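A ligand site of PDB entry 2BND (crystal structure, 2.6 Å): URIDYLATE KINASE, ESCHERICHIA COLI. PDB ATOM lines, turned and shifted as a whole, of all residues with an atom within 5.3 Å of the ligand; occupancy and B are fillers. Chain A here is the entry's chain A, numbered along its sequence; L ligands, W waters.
The side-chain carboxylate of Glu 19 lies close to an oxygen (O10) of the ligand (3.3 Å). An oxygen (O4) of the ligand sits close to the backbone carbonyl oxygen of Gly 80, at 3.3 Å. Residues that only touch the ligand: Gly 56 (3.3 Å), Phe 61 (3.99 Å), Thr 84 (3.7 Å), Gly 137 (3.9 Å), Pro 141 (3.5 Å), Phe 142 (3.8 Å) and Thr 144 (3.5 Å). Hydrophobic or aromatic side chains that line the ligand: Met 81 and Phe 143.
Water W2 lies within hydrogen-bond range of an oxygen (O5) of the ligand (3.0 Å), the backbone NH (N) of Ala 64 (3.2 Å) and the guanidinium group (NH2) of Arg 73 (3.4 Å). Water W3 lies within hydrogen-bond range of OG1 of Thr 145 (3.1 Å), N of Asp 146 (3.2 Å) and O11 of the ligand (3.2 Å). Water W1 lies within hydrogen-bond range of NH2 of Arg 73, OD1 of Asp 77 and O of Phe 143.
The backbone NH (N) of Gly 63 lies within hydrogen-bond range of an oxygen (O3) of the ligand (2.7 Å). NZ of Lys 15 lies within salt-bridge range of O11 of the ligand (2.6 Å). The side-chain hydroxyl of Ser 17 sits at hydrogen-bond distance from an oxygen (O10) of the ligand, 2.8 Å away. The backbone carbonyl oxygen of Asn 140 lies within hydrogen-bond range of a nitrogen (N2) of the ligand (2.7 Å). The backbone NH (N) of Thr 138 sits at hydrogen-bond distance from an oxygen (O2) of the ligand, 3.0 Å away. N of Gly 58 is in hydrogen-bond range of O10 of the ligand (2.9 Å). OD1 of Asp 77 lies within hydrogen-bond range of O3 of the ligand, at 2.6 Å. N of Gly 57 sits at hydrogen-bond distance from O9 of the ligand, 3.0 Å away. The guanidinium group (NH2) of Arg 62 is in salt-bridge range of an oxygen (O12) of the ligand, at 2.7 Å. The backbone NH (N) of Met 81 is in hydrogen-bond range of an oxygen (O4) of the ligand. OG1 of Thr 138 is in hydrogen-bond range of O2 of the ligand, 2.6 Å away. An oxygen (O10) of the ligand is in hydrogen-bond range of the backbone NH (N) of Gly 18 (2.7 Å). N2 of the ligand is in hydrogen-bond range of O of Phe 143 (2.9 Å). The backbone NH (N) of Thr 145 is in hydrogen-bond range of an oxygen (O8) of the ligand (2.8 Å). The side-chain hydroxyl (OG1) of Thr 145 is in hydrogen-bond range of an oxygen (O8) of the ligand (3.0 Å).
The side-chain hydroxyl of Thr 144 sits close to the backbone NH of Asp 146, 3.4 Å away. OG1 of Thr 84 is in hydrogen-bond range of N of Ala 136 (2.5 Å). The side-chain carboxylate (OE1) of Glu 19 lies within salt-bridge range of the guanidinium group (NH2) of Arg 62, at 3.0 Å. N of Gly 139 lies close to SD of Met 81. OD1 of Asp 77 is in salt-bridge range of NH2 of Arg 73, 2.9 Å away. The side-chain carboxylate (OD2) of Asp 77 sits at hydrogen-bond distance from the backbone NH (N) of Phe 142, at 2.6 Å. The side-chain amino group (NZ) of Lys 15 is in salt-bridge range of the side-chain carboxylate (OD1) of Asp 146 (3.4 Å). N of Asn 140 sits close to SD of Met 81, 3.7 Å away.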
ATOM      1  N   LYS A  15      36.457  -9.462   7.850  1.00  0.00           N
ATOM      2  CA  LYS A  15      35.829 -10.307   6.854  1.00  0.00           C
ATOM      3  C   LYS A  15      35.206 -11.506   7.570  1.00  0.00           C
ATOM      4  O   LYS A  15      35.917 -12.356   8.113  1.00  0.00           O
ATOM      5  CB  LYS A  15      36.867 -10.770   5.832  1.00  0.00           C
ATOM      6  CG  LYS A  15      36.275 -11.280   4.528  1.00  0.00           C
ATOM      7  CD  LYS A  15      35.513 -12.557   4.741  1.00  0.00           C
ATOM      8  CE  LYS A  15      34.977 -13.080   3.441  1.00  0.00           C
ATOM      9  NZ  LYS A  15      34.380 -14.409   3.628  1.00  0.00           N
ATOM     10  N   LEU A  16      33.880 -11.544   7.584  1.00  0.00           N
ATOM     11  CA  LEU A  16      33.149 -12.633   8.229  1.00  0.00           C
ATOM     12  C   LEU A  16      32.504 -13.477   7.159  1.00  0.00           C
ATOM     13  O   LEU A  16      31.588 -13.017   6.460  1.00  0.00           O
ATOM     14  CB  LEU A  16      32.064 -12.096   9.159  1.00  0.00           C
ATOM     15  CG  LEU A  16      32.468 -11.468  10.494  1.00  0.00           C
ATOM     16  CD1 LEU A  16      31.204 -11.062  11.240  1.00  0.00           C
ATOM     17  CD2 LEU A  16      33.269 -12.449  11.335  1.00  0.00           C
ATOM     18  N   SER A  17      32.972 -14.709   7.011  1.00  0.00           N
ATOM     19  CA  SER A  17      32.396 -15.617   6.031  1.00  0.00           C
ATOM     20  C   SER A  17      31.000 -16.025   6.488  1.00  0.00           C
ATOM     21  O   SER A  17      30.658 -15.887   7.662  1.00  0.00           O
ATOM     22  CB  SER A  17      33.282 -16.844   5.888  1.00  0.00           C
ATOM     23  OG  SER A  17      32.754 -17.728   4.912  1.00  0.00           O
ATOM     24  N   GLY A  18      30.185 -16.511   5.561  1.00  0.00           N
ATOM     25  CA  GLY A  18      28.837 -16.931   5.898  1.00  0.00           C
ATOM     26  C   GLY A  18      28.821 -18.050   6.915  1.00  0.00           C
ATOM     27  O   GLY A  18      28.047 -18.010   7.872  1.00  0.00           O
ATOM     28  N   GLU A  19      29.668 -19.059   6.719  1.00  0.00           N
ATOM     29  CA  GLU A  19      29.767 -20.207   7.628  1.00  0.00           C
ATOM     30  C   GLU A  19      29.803 -19.779   9.090  1.00  0.00           C
ATOM     31  O   GLU A  19      29.126 -20.364   9.932  1.00  0.00           O
ATOM     32  CB  GLU A  19      31.030 -21.024   7.325  1.00  0.00           C
ATOM     33  CG  GLU A  19      30.940 -22.004   6.166  1.00  0.00           C
ATOM     34  CD  GLU A  19      30.636 -21.334   4.835  1.00  0.00           C
ATOM     35  OE1 GLU A  19      31.288 -20.312   4.508  1.00  0.00           O
ATOM     36  OE2 GLU A  19      29.752 -21.838   4.120  1.00  0.00           O
ATOM     37  N   GLY A  56      29.900 -12.670   4.307  1.00  0.00           N
ATOM     38  CA  GLY A  56      29.638 -13.561   3.197  1.00  0.00           C
ATOM     39  C   GLY A  56      28.239 -14.138   3.201  1.00  0.00           C
ATOM     40  O   GLY A  56      27.352 -13.633   3.895  1.00  0.00           O
ATOM     41  N   GLY A  57      28.046 -15.216   2.431  1.00  0.00           N
ATOM     42  CA  GLY A  57      26.726 -15.834   2.350  1.00  0.00           C
ATOM     43  C   GLY A  57      26.703 -17.339   2.224  1.00  0.00           C
ATOM     44  O   GLY A  57      25.645 -17.935   1.985  1.00  0.00           O
ATOM     45  N   GLY A  58      27.862 -17.959   2.431  1.00  0.00           N
ATOM     46  CA  GLY A  58      27.980 -19.411   2.328  1.00  0.00           C
ATOM     47  C   GLY A  58      26.995 -20.238   3.136  1.00  0.00           C
ATOM     48  O   GLY A  58      26.743 -21.398   2.800  1.00  0.00           O
ATOM     49  N   ASN A  59      26.451 -19.655   4.198  1.00  0.00           N
ATOM     50  CA  ASN A  59      25.482 -20.360   5.041  1.00  0.00           C
ATOM     51  C   ASN A  59      24.107 -20.379   4.367  1.00  0.00           C
ATOM     52  O   ASN A  59      23.220 -21.129   4.774  1.00  0.00           O
ATOM     53  CB  ASN A  59      25.380 -19.674   6.395  1.00  0.00           C
ATOM     54  CG  ASN A  59      25.029 -18.214   6.279  1.00  0.00           C
ATOM     55  OD1 ASN A  59      25.649 -17.471   5.500  1.00  0.00           O
ATOM     56  ND2 ASN A  59      24.045 -17.764   7.050  1.00  0.00           N
ATOM     57  N   PHE A  61      23.545 -19.172   0.375  1.00  0.00           N
ATOM     58  CA  PHE A  61      23.706 -19.470  -1.040  1.00  0.00           C
ATOM     59  C   PHE A  61      25.033 -19.040  -1.640  1.00  0.00           C
ATOM     60  O   PHE A  61      25.669 -18.089  -1.182  1.00  0.00           O
ATOM     61  CB  PHE A  61      22.602 -18.789  -1.869  1.00  0.00           C
ATOM     62  CG  PHE A  61      21.204 -19.220  -1.540  1.00  0.00           C
ATOM     63  CD1 PHE A  61      20.405 -18.427  -0.714  1.00  0.00           C
ATOM     64  CD2 PHE A  61      20.683 -20.385  -2.073  1.00  0.00           C
ATOM     65  CE1 PHE A  61      19.091 -18.805  -0.422  1.00  0.00           C
ATOM     66  CE2 PHE A  61      19.378 -20.767  -1.795  1.00  0.00           C
ATOM     67  CZ  PHE A  61      18.584 -19.967  -0.974  1.00  0.00           C
ATOM     68  N   ARG A  62      25.439 -19.751  -2.682  1.00  0.00           N
ATOM     69  CA  ARG A  62      26.643 -19.437  -3.426  1.00  0.00           C
ATOM     70  C   ARG A  62      26.228 -19.539  -4.874  1.00  0.00           C
ATOM     71  O   ARG A  62      25.617 -20.525  -5.293  1.00  0.00           O
ATOM     72  CB  ARG A  62      27.766 -20.425  -3.107  1.00  0.00           C
ATOM     73  CG  ARG A  62      28.445 -20.167  -1.780  1.00  0.00           C
ATOM     74  CD  ARG A  62      29.890 -20.657  -1.820  1.00  0.00           C
ATOM     75  NE  ARG A  62      30.683 -20.226  -0.674  1.00  0.00           N
ATOM     76  CZ  ARG A  62      30.660 -20.803   0.525  1.00  0.00           C
ATOM     77  NH1 ARG A  62      29.871 -21.853   0.748  1.00  0.00           N
ATOM     78  NH2 ARG A  62      31.410 -20.333   1.499  1.00  0.00           N
ATOM     79  N   GLY A  63      26.519 -18.503  -5.647  1.00  0.00           N
ATOM     80  CA  GLY A  63      26.159 -18.499  -7.058  1.00  0.00           C
ATOM     81  C   GLY A  63      26.614 -19.719  -7.825  1.00  0.00           C
ATOM     82  O   GLY A  63      25.851 -20.277  -8.615  1.00  0.00           O
ATOM     83  N   ALA A  64      27.849 -20.148  -7.603  1.00  0.00           N
ATOM     84  CA  ALA A  64      28.361 -21.306  -8.327  1.00  0.00           C
ATOM     85  C   ALA A  64      27.478 -22.527  -8.073  1.00  0.00           C
ATOM     86  O   ALA A  64      27.016 -23.186  -9.021  1.00  0.00           O
ATOM     87  CB  ALA A  64      29.794 -21.600  -7.896  1.00  0.00           C
ATOM     88  N   ARG A  73      24.123 -18.283 -14.027  1.00  0.00           N
ATOM     89  CA  ARG A  73      25.174 -17.875 -13.121  1.00  0.00           C
ATOM     90  C   ARG A  73      24.947 -16.491 -12.522  1.00  0.00           C
ATOM     91  O   ARG A  73      25.082 -16.313 -11.313  1.00  0.00           O
ATOM     92  CB  ARG A  73      26.544 -17.908 -13.802  1.00  0.00           C
ATOM     93  CG  ARG A  73      27.668 -17.650 -12.818  1.00  0.00           C
ATOM     94  CD  ARG A  73      27.548 -18.596 -11.631  1.00  0.00           C
ATOM     95  NE  ARG A  73      28.229 -18.098 -10.441  1.00  0.00           N
ATOM     96  CZ  ARG A  73      29.556 -18.068 -10.290  1.00  0.00           C
ATOM     97  NH1 ARG A  73      30.351 -18.508 -11.251  1.00  0.00           N
ATOM     98  NH2 ARG A  73      30.074 -17.584  -9.175  1.00  0.00           N
ATOM     99  N   GLY A  76      22.383 -16.505  -9.966  1.00  0.00           N
ATOM    100  CA  GLY A  76      22.855 -17.227  -8.813  1.00  0.00           C
ATOM    101  C   GLY A  76      23.657 -16.283  -7.934  1.00  0.00           C
ATOM    102  O   GLY A  76      23.420 -16.179  -6.731  1.00  0.00           O
ATOM    103  N   ASP A  77      24.602 -15.575  -8.546  1.00  0.00           N
ATOM    104  CA  ASP A  77      25.440 -14.624  -7.813  1.00  0.00           C
ATOM    105  C   ASP A  77      24.616 -13.478  -7.242  1.00  0.00           C
ATOM    106  O   ASP A  77      25.011 -12.836  -6.270  1.00  0.00           O
ATOM    107  CB  ASP A  77      26.560 -14.092  -8.718  1.00  0.00           C
ATOM    108  CG  ASP A  77      27.662 -15.126  -8.966  1.00  0.00           C
ATOM    109  OD1 ASP A  77      27.742 -16.118  -8.208  1.00  0.00           O
ATOM    110  OD2 ASP A  77      28.465 -14.952  -9.910  1.00  0.00           O
ATOM    111  N   HIS A  78      23.458 -13.208  -7.839  1.00  0.00           N
ATOM    112  CA  HIS A  78      22.614 -12.140  -7.332  1.00  0.00           C
ATOM    113  C   HIS A  78      22.015 -12.624  -6.005  1.00  0.00           C
ATOM    114  O   HIS A  78      22.191 -11.993  -4.970  1.00  0.00           O
ATOM    115  CB  HIS A  78      21.511 -11.781  -8.340  1.00  0.00           C
ATOM    116  CG  HIS A  78      21.960 -10.818  -9.407  1.00  0.00           C
ATOM    117  ND1 HIS A  78      21.160 -10.474 -10.480  1.00  0.00           N
ATOM    118  CD2 HIS A  78      23.131 -10.155  -9.583  1.00  0.00           C
ATOM    119  CE1 HIS A  78      21.824  -9.634 -11.261  1.00  0.00           C
ATOM    120  NE2 HIS A  78      23.011  -9.425 -10.739  1.00  0.00           N
ATOM    121  N   GLY A  80      22.990 -14.899  -4.168  1.00  0.00           N
ATOM    122  CA  GLY A  80      24.065 -15.060  -3.208  1.00  0.00           C
ATOM    123  C   GLY A  80      24.394 -13.728  -2.569  1.00  0.00           C
ATOM    124  O   GLY A  80      24.692 -13.651  -1.375  1.00  0.00           O
ATOM    125  N   MET A  81      24.352 -12.660  -3.364  1.00  0.00           N
ATOM    126  CA  MET A  81      24.643 -11.347  -2.829  1.00  0.00           C
ATOM    127  C   MET A  81      23.541 -10.970  -1.849  1.00  0.00           C
ATOM    128  O   MET A  81      23.816 -10.536  -0.726  1.00  0.00           O
ATOM    129  CB  MET A  81      24.768 -10.310  -3.952  1.00  0.00           C
ATOM    130  CG  MET A  81      26.025 -10.505  -4.807  1.00  0.00           C
ATOM    131  SD  MET A  81      26.637  -9.023  -5.637  1.00  0.00           S
ATOM    132  CE  MET A  81      26.017  -9.240  -7.276  1.00  0.00           C
ATOM    133  N   THR A  84      24.253 -12.187   1.453  1.00  0.00           N
ATOM    134  CA  THR A  84      25.189 -11.420   2.268  1.00  0.00           C
ATOM    135  C   THR A  84      24.399 -10.336   2.990  1.00  0.00           C
ATOM    136  O   THR A  84      24.594 -10.087   4.179  1.00  0.00           O
ATOM    137  CB  THR A  84      26.295 -10.740   1.423  1.00  0.00           C
ATOM    138  OG1 THR A  84      25.703  -9.791   0.529  1.00  0.00           O
ATOM    139  CG2 THR A  84      27.064 -11.766   0.615  1.00  0.00           C
ATOM    140  N   ALA A 136      26.191  -7.337   0.288  1.00  0.00           N
ATOM    141  CA  ALA A 136      26.051  -7.429  -1.166  1.00  0.00           C
ATOM    142  C   ALA A 136      27.400  -7.409  -1.860  1.00  0.00           C
ATOM    143  O   ALA A 136      27.493  -7.161  -3.056  1.00  0.00           O
ATOM    144  CB  ALA A 136      25.175  -6.297  -1.699  1.00  0.00           C
ATOM    145  N   GLY A 137      28.462  -7.661  -1.089  1.00  0.00           N
ATOM    146  CA  GLY A 137      29.799  -7.694  -1.651  1.00  0.00           C
ATOM    147  C   GLY A 137      30.220  -6.505  -2.497  1.00  0.00           C
ATOM    148  O   GLY A 137      30.084  -5.352  -2.097  1.00  0.00           O
ATOM    149  N   THR A 138      30.766  -6.805  -3.679  1.00  0.00           N
ATOM    150  CA  THR A 138      31.207  -5.785  -4.604  1.00  0.00           C
ATOM    151  C   THR A 138      30.019  -5.336  -5.450  1.00  0.00           C
ATOM    152  O   THR A 138      30.062  -4.303  -6.103  1.00  0.00           O
ATOM    153  CB  THR A 138      32.292  -6.352  -5.555  1.00  0.00           C
ATOM    154  OG1 THR A 138      31.699  -7.349  -6.396  1.00  0.00           O
ATOM    155  CG2 THR A 138      33.428  -6.977  -4.775  1.00  0.00           C
ATOM    156  N   GLY A 139      28.956  -6.138  -5.436  1.00  0.00           N
ATOM    157  CA  GLY A 139      27.766  -5.804  -6.198  1.00  0.00           C
ATOM    158  C   GLY A 139      27.745  -6.432  -7.570  1.00  0.00           C
ATOM    159  O   GLY A 139      26.742  -6.344  -8.273  1.00  0.00           O
ATOM    160  N   ASN A 140      28.831  -7.080  -7.962  1.00  0.00           N
ATOM    161  CA  ASN A 140      28.934  -7.725  -9.263  1.00  0.00           C
ATOM    162  C   ASN A 140      29.002  -9.246  -9.176  1.00  0.00           C
ATOM    163  O   ASN A 140      29.497  -9.810  -8.205  1.00  0.00           O
ATOM    164  CB  ASN A 140      30.194  -7.257 -10.003  1.00  0.00           C
ATOM    165  CG  ASN A 140      30.107  -5.823 -10.454  1.00  0.00           C
ATOM    166  OD1 ASN A 140      29.223  -5.458 -11.221  1.00  0.00           O
ATOM    167  ND2 ASN A 140      31.028  -4.989  -9.977  1.00  0.00           N
ATOM    168  N   PRO A 141      28.504  -9.941 -10.209  1.00  0.00           N
ATOM    169  CA  PRO A 141      28.548 -11.408 -10.216  1.00  0.00           C
ATOM    170  C   PRO A 141      29.988 -11.842 -10.500  1.00  0.00           C
ATOM    171  O   PRO A 141      30.824 -11.029 -10.900  1.00  0.00           O
ATOM    172  CB  PRO A 141      27.590 -11.785 -11.350  1.00  0.00           C
ATOM    173  CG  PRO A 141      27.735 -10.631 -12.284  1.00  0.00           C
ATOM    174  CD  PRO A 141      27.700  -9.445 -11.345  1.00  0.00           C
ATOM    175  N   PHE A 142      30.286 -13.124 -10.309  1.00  0.00           N
ATOM    176  CA  PHE A 142      31.622 -13.665 -10.550  1.00  0.00           C
ATOM    177  C   PHE A 142      32.645 -13.095  -9.585  1.00  0.00           C
ATOM    178  O   PHE A 142      33.805 -12.934  -9.930  1.00  0.00           O
ATOM    179  CB  PHE A 142      32.078 -13.366 -11.994  1.00  0.00           C
ATOM    180  CG  PHE A 142      31.092 -13.796 -13.034  1.00  0.00           C
ATOM    181  CD1 PHE A 142      30.800 -15.133 -13.231  1.00  0.00           C
ATOM    182  CD2 PHE A 142      30.413 -12.835 -13.790  1.00  0.00           C
ATOM    183  CE1 PHE A 142      29.836 -15.530 -14.167  1.00  0.00           C
ATOM    184  CE2 PHE A 142      29.452 -13.213 -14.735  1.00  0.00           C
ATOM    185  CZ  PHE A 142      29.167 -14.572 -14.914  1.00  0.00           C
ATOM    186  N   PHE A 143      32.216 -12.770  -8.381  1.00  0.00           N
ATOM    187  CA  PHE A 143      33.127 -12.241  -7.373  1.00  0.00           C
ATOM    188  C   PHE A 143      32.778 -12.852  -6.020  1.00  0.00           C
ATOM    189  O   PHE A 143      31.673 -13.349  -5.813  1.00  0.00           O
ATOM    190  CB  PHE A 143      33.058 -10.716  -7.299  1.00  0.00           C
ATOM    191  CG  PHE A 143      33.910 -10.010  -8.325  1.00  0.00           C
ATOM    192  CD1 PHE A 143      33.323  -9.319  -9.369  1.00  0.00           C
ATOM    193  CD2 PHE A 143      35.293 -10.079  -8.261  1.00  0.00           C
ATOM    194  CE1 PHE A 143      34.108  -8.707 -10.351  1.00  0.00           C
ATOM    195  CE2 PHE A 143      36.084  -9.476  -9.229  1.00  0.00           C
ATOM    196  CZ  PHE A 143      35.493  -8.788 -10.281  1.00  0.00           C
ATOM    197  N   THR A 144      33.744 -12.828  -5.114  1.00  0.00           N
ATOM    198  CA  THR A 144      33.556 -13.390  -3.780  1.00  0.00           C
ATOM    199  C   THR A 144      33.537 -12.268  -2.751  1.00  0.00           C
ATOM    200  O   THR A 144      34.099 -11.201  -3.000  1.00  0.00           O
ATOM    201  CB  THR A 144      34.705 -14.337  -3.419  1.00  0.00           C
ATOM    202  OG1 THR A 144      35.938 -13.599  -3.432  1.00  0.00           O
ATOM    203  CG2 THR A 144      34.771 -15.484  -4.411  1.00  0.00           C
ATOM    204  N   THR A 145      32.914 -12.494  -1.605  1.00  0.00           N
ATOM    205  CA  THR A 145      32.908 -11.446  -0.598  1.00  0.00           C
ATOM    206  C   THR A 145      34.345 -11.176  -0.139  1.00  0.00           C
ATOM    207  O   THR A 145      34.613 -10.120   0.432  1.00  0.00           O
ATOM    208  CB  THR A 145      32.028 -11.787   0.613  1.00  0.00           C
ATOM    209  OG1 THR A 145      32.403 -13.051   1.161  1.00  0.00           O
ATOM    210  CG2 THR A 145      30.568 -11.799   0.207  1.00  0.00           C
ATOM    211  N   ASP A 146      35.255 -12.109  -0.405  1.00  0.00           N
ATOM    212  CA  ASP A 146      36.651 -11.893  -0.057  1.00  0.00           C
ATOM    213  C   ASP A 146      37.181 -10.688  -0.864  1.00  0.00           C
ATOM    214  O   ASP A 146      37.870  -9.834  -0.318  1.00  0.00           O
ATOM    215  CB  ASP A 146      37.501 -13.135  -0.354  1.00  0.00           C
ATOM    216  CG  ASP A 146      37.598 -14.091   0.837  1.00  0.00           C
ATOM    217  OD1 ASP A 146      37.250 -13.700   1.978  1.00  0.00           O
ATOM    218  OD2 ASP A 146      38.044 -15.238   0.639  1.00  0.00           O
ATOM    219  N   ALA A 148      35.391  -8.350  -2.109  1.00  0.00           N
ATOM    220  CA  ALA A 148      34.683  -7.224  -1.498  1.00  0.00           C
ATOM    221  C   ALA A 148      35.487  -6.754  -0.291  1.00  0.00           C
ATOM    222  O   ALA A 148      35.689  -5.552  -0.091  1.00  0.00           O
ATOM    223  CB  ALA A 148      33.269  -7.666  -1.065  1.00  0.00           C
HETATM  224  N1  LIG L   1      28.842 -12.634  -4.629  1.00  0.00           N
HETATM  225  C1  LIG L   1      29.075 -12.056  -5.896  1.00  0.00           C
HETATM  226  N2  LIG L   1      30.013 -11.017  -5.897  1.00  0.00           N
HETATM  227  C2  LIG L   1      30.637 -10.442  -4.785  1.00  0.00           C
HETATM  228  C3  LIG L   1      30.327 -11.048  -3.521  1.00  0.00           C
HETATM  229  C4  LIG L   1      29.474 -12.097  -3.481  1.00  0.00           C
HETATM  230  O1  LIG L   1      28.601 -12.510  -6.925  1.00  0.00           O
HETATM  231  O2  LIG L   1      31.359  -9.458  -4.951  1.00  0.00           O
HETATM  232  C5  LIG L   1      27.911 -13.804  -4.575  1.00  0.00           C
HETATM  233  C6  LIG L   1      28.541 -15.157  -4.917  1.00  0.00           C
HETATM  234  O3  LIG L   1      27.616 -15.983  -5.583  1.00  0.00           O
HETATM  235  C7  LIG L   1      28.960 -15.697  -3.550  1.00  0.00           C
HETATM  236  C8  LIG L   1      27.905 -15.111  -2.620  1.00  0.00           C
HETATM  237  O4  LIG L   1      27.337 -13.952  -3.297  1.00  0.00           O
HETATM  238  O5  LIG L   1      28.961 -17.113  -3.478  1.00  0.00           O
HETATM  239  C9  LIG L   1      28.448 -14.674  -1.287  1.00  0.00           C
HETATM  240  O6  LIG L   1      29.051 -15.773  -0.673  1.00  0.00           O
HETATM  241  P1  LIG L   1      30.628 -15.925  -0.586  1.00  0.00           P
HETATM  242  O7  LIG L   1      31.026 -17.256  -1.130  1.00  0.00           O
HETATM  243  O8  LIG L   1      31.301 -14.686  -1.060  1.00  0.00           O
HETATM  244  O9  LIG L   1      30.658 -15.894   1.022  1.00  0.00           O
HETATM  245  P2  LIG L   1      31.471 -16.664   2.107  1.00  0.00           P
HETATM  246  O10 LIG L   1      30.668 -17.387   3.085  1.00  0.00           O
HETATM  247  O11 LIG L   1      32.398 -15.686   2.580  1.00  0.00           O
HETATM  248  O12 LIG L   1      32.224 -17.750   1.226  1.00  0.00           O
HETATM  249  O   HOH W   1      30.704 -15.758  -7.602  1.00  0.00           O
HETATM  250  O   HOH W   2      30.011 -18.421  -5.922  1.00  0.00           O
HETATM  251  O   HOH W   3      34.365 -15.142   0.067  1.00  0.00           O
